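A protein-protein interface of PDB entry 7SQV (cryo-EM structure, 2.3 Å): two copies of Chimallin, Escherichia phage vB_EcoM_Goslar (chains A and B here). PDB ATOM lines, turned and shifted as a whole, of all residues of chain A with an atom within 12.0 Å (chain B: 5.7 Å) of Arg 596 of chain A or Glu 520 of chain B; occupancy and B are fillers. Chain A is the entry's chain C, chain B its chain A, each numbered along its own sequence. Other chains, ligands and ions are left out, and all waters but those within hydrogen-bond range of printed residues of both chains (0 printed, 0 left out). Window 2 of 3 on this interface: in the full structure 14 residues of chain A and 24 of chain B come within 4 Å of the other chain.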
ATOM      1  N   ALA A 594      -7.858  12.474  21.973  1.00  0.00           N
ATOM      2  CA  ALA A 594      -8.681  13.465  21.289  1.00  0.00           C
ATOM      3  C   ALA A 594      -7.814  14.542  20.643  1.00  0.00           C
ATOM      4  O   ALA A 594      -6.607  14.366  20.480  1.00  0.00           O
ATOM      5  CB  ALA A 594      -9.672  14.091  22.257  1.00  0.00           C
ATOM      6  N   VAL A 595      -8.440  15.657  20.277  1.00  0.00           N
ATOM      7  CA  VAL A 595      -7.758  16.781  19.646  1.00  0.00           C
ATOM      8  C   VAL A 595      -7.950  18.013  20.520  1.00  0.00           C
ATOM      9  O   VAL A 595      -9.079  18.338  20.907  1.00  0.00           O
ATOM     10  CB  VAL A 595      -8.275  17.034  18.218  1.00  0.00           C
ATOM     11  CG1 VAL A 595      -7.595  16.092  17.237  1.00  0.00           C
ATOM     12  CG2 VAL A 595      -9.785  16.863  18.160  1.00  0.00           C
ATOM     13  N   ARG A 596      -6.848  18.686  20.837  1.00  0.00           N
ATOM     14  CA  ARG A 596      -6.895  19.888  21.651  1.00  0.00           C
ATOM     15  C   ARG A 596      -7.383  21.078  20.830  1.00  0.00           C
ATOM     16  O   ARG A 596      -7.388  21.058  19.596  1.00  0.00           O
ATOM     17  CB  ARG A 596      -5.516  20.189  22.240  1.00  0.00           C
ATOM     18  CG  ARG A 596      -4.990  19.111  23.171  1.00  0.00           C
ATOM     19  CD  ARG A 596      -3.715  19.562  23.865  1.00  0.00           C
ATOM     20  NE  ARG A 596      -3.917  20.781  24.638  1.00  0.00           N
ATOM     21  CZ  ARG A 596      -3.277  21.921  24.418  1.00  0.00           C
ATOM     22  NH1 ARG A 596      -2.383  22.036  23.450  1.00  0.00           N
ATOM     23  NH2 ARG A 596      -3.542  22.973  25.188  1.00  0.00           N
ATOM     24  N   GLY A 597      -7.795  22.122  21.533  1.00  0.00           N
ATOM     25  CA  GLY A 597      -8.213  23.362  20.916  1.00  0.00           C
ATOM     26  C   GLY A 597      -9.717  23.571  21.002  1.00  0.00           C
ATOM     27  O   GLY A 597     -10.492  22.669  21.322  1.00  0.00           O
ATOM     28  N   ASN A 598     -10.115  24.805  20.703  1.00  0.00           N
ATOM     29  CA  ASN A 598     -11.514  25.219  20.698  1.00  0.00           C
ATOM     30  C   ASN A 598     -11.914  25.522  19.259  1.00  0.00           C
ATOM     31  O   ASN A 598     -11.404  26.472  18.654  1.00  0.00           O
ATOM     32  CB  ASN A 598     -11.726  26.432  21.599  1.00  0.00           C
ATOM     33  CG  ASN A 598     -13.191  26.760  21.803  1.00  0.00           C
ATOM     34  OD1 ASN A 598     -14.072  25.992  21.416  1.00  0.00           O
ATOM     35  ND2 ASN A 598     -13.461  27.907  22.415  1.00  0.00           N
ATOM     36  N   MET A 599     -12.824  24.716  18.713  1.00  0.00           N
ATOM     37  CA  MET A 599     -13.237  24.866  17.322  1.00  0.00           C
ATOM     38  C   MET A 599     -14.329  25.909  17.133  1.00  0.00           C
ATOM     39  O   MET A 599     -14.422  26.506  16.053  1.00  0.00           O
ATOM     40  CB  MET A 599     -13.719  23.522  16.770  1.00  0.00           C
ATOM     41  CG  MET A 599     -12.604  22.529  16.488  1.00  0.00           C
ATOM     42  SD  MET A 599     -11.033  23.329  16.110  1.00  0.00           S
ATOM     43  CE  MET A 599      -9.898  22.310  17.050  1.00  0.00           C
ATOM     44  N   ALA A 600     -15.157  26.145  18.151  1.00  0.00           N
ATOM     45  CA  ALA A 600     -16.257  27.092  18.023  1.00  0.00           C
ATOM     46  C   ALA A 600     -15.804  28.543  18.089  1.00  0.00           C
ATOM     47  O   ALA A 600     -16.533  29.426  17.621  1.00  0.00           O
ATOM     48  CB  ALA A 600     -17.303  26.834  19.110  1.00  0.00           C
ATOM     49  N   ALA A 601     -14.625  28.814  18.655  1.00  0.00           N
ATOM     50  CA  ALA A 601     -14.164  30.193  18.781  1.00  0.00           C
ATOM     51  C   ALA A 601     -13.814  30.800  17.429  1.00  0.00           C
ATOM     52  O   ALA A 601     -13.979  32.009  17.235  1.00  0.00           O
ATOM     53  CB  ALA A 601     -12.961  30.260  19.720  1.00  0.00           C
ATOM     54  N   ARG A 602     -13.325  29.985  16.492  1.00  0.00           N
ATOM     55  CA  ARG A 602     -12.927  30.503  15.188  1.00  0.00           C
ATOM     56  C   ARG A 602     -14.120  31.048  14.411  1.00  0.00           C
ATOM     57  O   ARG A 602     -14.007  32.071  13.727  1.00  0.00           O
ATOM     58  CB  ARG A 602     -12.220  29.409  14.389  1.00  0.00           C
ATOM     59  CG  ARG A 602     -11.579  29.886  13.100  1.00  0.00           C
ATOM     60  CD  ARG A 602     -11.023  28.715  12.308  1.00  0.00           C
ATOM     61  NE  ARG A 602     -10.843  27.533  13.143  1.00  0.00           N
ATOM     62  CZ  ARG A 602     -10.794  26.291  12.684  1.00  0.00           C
ATOM     63  NH1 ARG A 602     -10.910  26.025  11.394  1.00  0.00           N
ATOM     64  NH2 ARG A 602     -10.626  25.288  13.542  1.00  0.00           N
ATOM     65  N   TYR B 295      -6.424  29.215  21.796  1.00  0.00           N
ATOM     66  CA  TYR B 295      -5.860  28.190  20.928  1.00  0.00           C
ATOM     67  C   TYR B 295      -6.952  27.579  20.059  1.00  0.00           C
ATOM     68  O   TYR B 295      -8.006  27.174  20.559  1.00  0.00           O
ATOM     69  CB  TYR B 295      -5.176  27.112  21.767  1.00  0.00           C
ATOM     70  CG  TYR B 295      -4.494  26.029  20.961  1.00  0.00           C
ATOM     71  CD1 TYR B 295      -3.511  26.342  20.033  1.00  0.00           C
ATOM     72  CD2 TYR B 295      -4.825  24.693  21.141  1.00  0.00           C
ATOM     73  CE1 TYR B 295      -2.882  25.354  19.298  1.00  0.00           C
ATOM     74  CE2 TYR B 295      -4.202  23.699  20.412  1.00  0.00           C
ATOM     75  CZ  TYR B 295      -3.233  24.034  19.492  1.00  0.00           C
ATOM     76  OH  TYR B 295      -2.610  23.047  18.765  1.00  0.00           O
ATOM     77  N   PRO B 297      -6.375  25.342  16.555  1.00  0.00           N
ATOM     78  CA  PRO B 297      -5.680  24.857  15.359  1.00  0.00           C
ATOM     79  C   PRO B 297      -6.648  24.484  14.248  1.00  0.00           C
ATOM     80  O   PRO B 297      -7.794  24.099  14.489  1.00  0.00           O
ATOM     81  CB  PRO B 297      -4.921  23.628  15.869  1.00  0.00           C
ATOM     82  CG  PRO B 297      -5.746  23.140  17.009  1.00  0.00           C
ATOM     83  CD  PRO B 297      -6.320  24.372  17.660  1.00  0.00           C
ATOM     84  N   ASN B 515       6.498  27.105  32.205  1.00  0.00           N
ATOM     85  CA  ASN B 515       6.877  26.034  31.298  1.00  0.00           C
ATOM     86  C   ASN B 515       5.690  25.612  30.440  1.00  0.00           C
ATOM     87  O   ASN B 515       4.538  25.911  30.766  1.00  0.00           O
ATOM     88  CB  ASN B 515       7.410  24.845  32.096  1.00  0.00           C
ATOM     89  CG  ASN B 515       6.449  24.387  33.172  1.00  0.00           C
ATOM     90  OD1 ASN B 515       5.566  23.568  32.923  1.00  0.00           O
ATOM     91  ND2 ASN B 515       6.617  24.913  34.379  1.00  0.00           N
ATOM     92  N   PRO B 516       5.941  24.925  29.320  1.00  0.00           N
ATOM     93  CA  PRO B 516       4.826  24.547  28.431  1.00  0.00           C
ATOM     94  C   PRO B 516       3.775  23.660  29.082  1.00  0.00           C
ATOM     95  O   PRO B 516       2.622  23.671  28.635  1.00  0.00           O
ATOM     96  CB  PRO B 516       5.530  23.822  27.271  1.00  0.00           C
ATOM     97  CG  PRO B 516       6.926  23.549  27.748  1.00  0.00           C
ATOM     98  CD  PRO B 516       7.247  24.646  28.701  1.00  0.00           C
ATOM     99  N   ASP B 517       4.132  22.881  30.106  1.00  0.00           N
ATOM    100  CA  ASP B 517       3.136  22.045  30.773  1.00  0.00           C
ATOM    101  C   ASP B 517       2.059  22.895  31.438  1.00  0.00           C
ATOM    102  O   ASP B 517       0.865  22.573  31.360  1.00  0.00           O
ATOM    103  CB  ASP B 517       3.810  21.138  31.801  1.00  0.00           C
ATOM    104  CG  ASP B 517       4.722  20.110  31.162  1.00  0.00           C
ATOM    105  OD1 ASP B 517       4.787  20.062  29.917  1.00  0.00           O
ATOM    106  OD2 ASP B 517       5.377  19.350  31.908  1.00  0.00           O
ATOM    107  N   THR B 518       2.462  23.983  32.097  1.00  0.00           N
ATOM    108  CA  THR B 518       1.490  24.880  32.714  1.00  0.00           C
ATOM    109  C   THR B 518       0.597  25.529  31.665  1.00  0.00           C
ATOM    110  O   THR B 518      -0.611  25.689  31.879  1.00  0.00           O
ATOM    111  CB  THR B 518       2.211  25.945  33.540  1.00  0.00           C
ATOM    112  OG1 THR B 518       3.213  25.323  34.354  1.00  0.00           O
ATOM    113  CG2 THR B 518       1.227  26.684  34.434  1.00  0.00           C
ATOM    114  N   VAL B 519       1.175  25.913  30.524  1.00  0.00           N
ATOM    115  CA  VAL B 519       0.385  26.495  29.442  1.00  0.00           C
ATOM    116  C   VAL B 519      -0.637  25.491  28.930  1.00  0.00           C
ATOM    117  O   VAL B 519      -1.804  25.833  28.689  1.00  0.00           O
ATOM    118  CB  VAL B 519       1.310  26.986  28.313  1.00  0.00           C
ATOM    119  CG1 VAL B 519       0.497  27.621  27.196  1.00  0.00           C
ATOM    120  CG2 VAL B 519       2.342  27.961  28.857  1.00  0.00           C
ATOM    121  N   GLU B 520      -0.215  24.238  28.744  1.00  0.00           N
ATOM    122  CA  GLU B 520      -1.135  23.203  28.287  1.00  0.00           C
ATOM    123  C   GLU B 520      -2.260  22.982  29.289  1.00  0.00           C
ATOM    124  O   GLU B 520      -3.424  22.843  28.900  1.00  0.00           O
ATOM    125  CB  GLU B 520      -0.376  21.900  28.040  1.00  0.00           C
ATOM    126  CG  GLU B 520      -1.071  20.954  27.076  1.00  0.00           C
ATOM    127  CD  GLU B 520      -0.596  19.523  27.222  1.00  0.00           C
ATOM    128  OE1 GLU B 520      -1.286  18.734  27.902  1.00  0.00           O
ATOM    129  OE2 GLU B 520       0.467  19.188  26.660  1.00  0.00           O
ATOM    130  N   ALA B 521      -1.930  22.946  30.582  1.00  0.00           N
ATOM    131  CA  ALA B 521      -2.961  22.765  31.601  1.00  0.00           C
ATOM    132  C   ALA B 521      -3.945  23.930  31.608  1.00  0.00           C
ATOM    133  O   ALA B 521      -5.160  23.726  31.715  1.00  0.00           O
ATOM    134  CB  ALA B 521      -2.317  22.597  32.977  1.00  0.00           C
ATOM    135  N   TRP B 522      -3.435  25.159  31.493  1.00  0.00           N
ATOM    136  CA  TRP B 522      -4.298  26.337  31.462  1.00  0.00           C
ATOM    137  C   TRP B 522      -5.241  26.293  30.264  1.00  0.00           C
ATOM    138  O   TRP B 522      -6.454  26.514  30.397  1.00  0.00           O
ATOM    139  CB  TRP B 522      -3.427  27.595  31.427  1.00  0.00           C
ATOM    140  CG  TRP B 522      -4.158  28.887  31.601  1.00  0.00           C
ATOM    141  CD1 TRP B 522      -4.559  29.741  30.614  1.00  0.00           C
ATOM    142  CD2 TRP B 522      -4.543  29.496  32.838  1.00  0.00           C
ATOM    143  NE1 TRP B 522      -5.186  30.834  31.159  1.00  0.00           N
ATOM    144  CE2 TRP B 522      -5.188  30.709  32.523  1.00  0.00           C
ATOM    145  CE3 TRP B 522      -4.413  29.130  34.181  1.00  0.00           C
ATOM    146  CZ2 TRP B 522      -5.701  31.557  33.502  1.00  0.00           C
ATOM    147  CZ3 TRP B 522      -4.923  29.973  35.150  1.00  0.00           C
ATOM    148  CH2 TRP B 522      -5.560  31.172  34.806  1.00  0.00           C
ATOM    149  N   GLU B 523      -4.698  25.994  29.080  1.00  0.00           N
ATOM    150  CA  GLU B 523      -5.523  25.937  27.879  1.00  0.00           C
ATOM    151  C   GLU B 523      -6.554  24.818  27.963  1.00  0.00           C
ATOM    152  O   GLU B 523      -7.703  24.992  27.541  1.00  0.00           O
ATOM    153  CB  GLU B 523      -4.641  25.768  26.642  1.00  0.00           C
ATOM    154  CG  GLU B 523      -3.923  27.039  26.221  1.00  0.00           C
ATOM    155  CD  GLU B 523      -2.916  26.802  25.114  1.00  0.00           C
ATOM    156  OE1 GLU B 523      -2.660  25.625  24.781  1.00  0.00           O
ATOM    157  OE2 GLU B 523      -2.380  27.792  24.574  1.00  0.00           O
ATOM    158  N   ASP B 524      -6.161  23.658  28.495  1.00  0.00           N
ATOM    159  CA  ASP B 524      -7.105  22.556  28.642  1.00  0.00           C
ATOM    160  C   ASP B 524      -8.226  22.915  29.607  1.00  0.00           C
ATOM    161  O   ASP B 524      -9.397  22.609  29.352  1.00  0.00           O
ATOM    162  CB  ASP B 524      -6.376  21.297  29.108  1.00  0.00           C
ATOM    163  CG  ASP B 524      -5.841  20.475  27.954  1.00  0.00           C
ATOM    164  OD1 ASP B 524      -5.820  20.990  26.816  1.00  0.00           O
ATOM    165  OD2 ASP B 524      -5.443  19.314  28.184  1.00  0.00           O
ATOM    166  N   SER B 525      -7.890  23.566  30.724  1.00  0.00           N
ATOM    167  CA  SER B 525      -8.920  24.014  31.651  1.00  0.00           C
ATOM    168  C   SER B 525      -9.860  25.023  31.011  1.00  0.00           C
ATOM    169  O   SER B 525     -11.060  25.009  31.307  1.00  0.00           O
ATOM    170  CB  SER B 525      -8.282  24.625  32.899  1.00  0.00           C
ATOM    171  OG  SER B 525      -7.691  25.878  32.605  1.00  0.00           O
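O of Tyr 295 of chain B lies within hydrogen-bond range of N of Asn 598 of chain A (3.2 Å). The backbone carbonyl oxygen (O) of Pro 297 of chain B sits at hydrogen-bond distance from the guanidinium group (NH2) of Arg 602 of chain A (3.2 Å). OE1 of Glu 523 of chain B is in salt-bridge range of NH2 of Arg 596 of chain A. SD of Met 599 of chain A sits close to O of Pro 297 of chain B (3.7 Å). The side-chain carboxylate (OD1) of Asp 524 of chain B lies within salt-bridge range of the guanidinium group (NE) of Arg 596 of chain A, 2.9 Å away.
The guanidinium group (NH2) of Arg 602 of chain A sits at hydrogen-bond distance from the side-chain sulfur (SD) of Met 599 of chain A (3.3 Å). The backbone NH (N) of Ala 600 of chain A is in hydrogen-bond range of the side-chain amide oxygen (OD1) of Asn 598 of chain A, 3.4 Å away.
Among the printed residues, pairs that only touch across the chains: Arg 596 of chain A with Tyr 295 of chain B (3.9 Å), Arg 596 of chain A with Pro 297 of chain B (3.7 Å), Arg 596 of chain A with Glu 520 of chain B (3.6 Å), Gly 597 of chain A with Tyr 295 of chain B (3.6 Å) and Gly 597 of chain A with Pro 297 of chain B (3.9 Å).
Glu 520 of chain B touches just one residue of chain A: Arg 596 (3.6 Å). Of chain A, only Arg 596, Gly 597 and Asn 598 come within 4 Å of Tyr 295 of chain B. Of chain A, only Arg 596 (3.7 Å), Gly 597 (3.9 Å), Met 599 (3.7 Å) and Arg 602 (3.2 Å) come within 4 Å of Pro 297 of chain B. No residue of chain A comes within 4 Å of Pro 516 of chain B. No residue of chain A comes within 4 Å of Asp 517 of chain B. No residue of chain A comes within 4 Å of Ala 521 of chain B. Asp 524 of chain B touches one residue of chain A. Of the printed residues of chain B, Asn 598 of chain A touches Tyr 295 (3.2 Å). Of the printed residues of chain B, Arg 602 of chain A touches Pro 297. Of the printed residues of chain B, Gly 597 of chain A touches Tyr 295 and Pro 297. Ala 594 of chain A touches none of the printed residues of chain B. Ser 525 of chain B touches none of the printed residues of chain A. The nearest residue of chain B that does not touch Arg 596 of chain A is Val 519 of chain B (4.8 Å). The nearest residue of chain A that does not touch Glu 520 of chain B is Gly 597 of chain A (8.6 Å).
Of the 13 printed residues of chain B, 5 touch a printed residue of chain A. Hydrophobic or aromatic side chains of chain B within 4 Å of the printed part of chain A: Tyr 295 and Pro 297. Among the printed residues, Asp or Glu carboxylates within 4 Å of a Lys or Arg side-chain nitrogen of the other chain: Arg 596 of chain A with Glu 523 of chain B (2.8 Å) and Arg 596 of chain A with Asp 524 of chain B (2.9 Å).
No position is printed for both chains.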
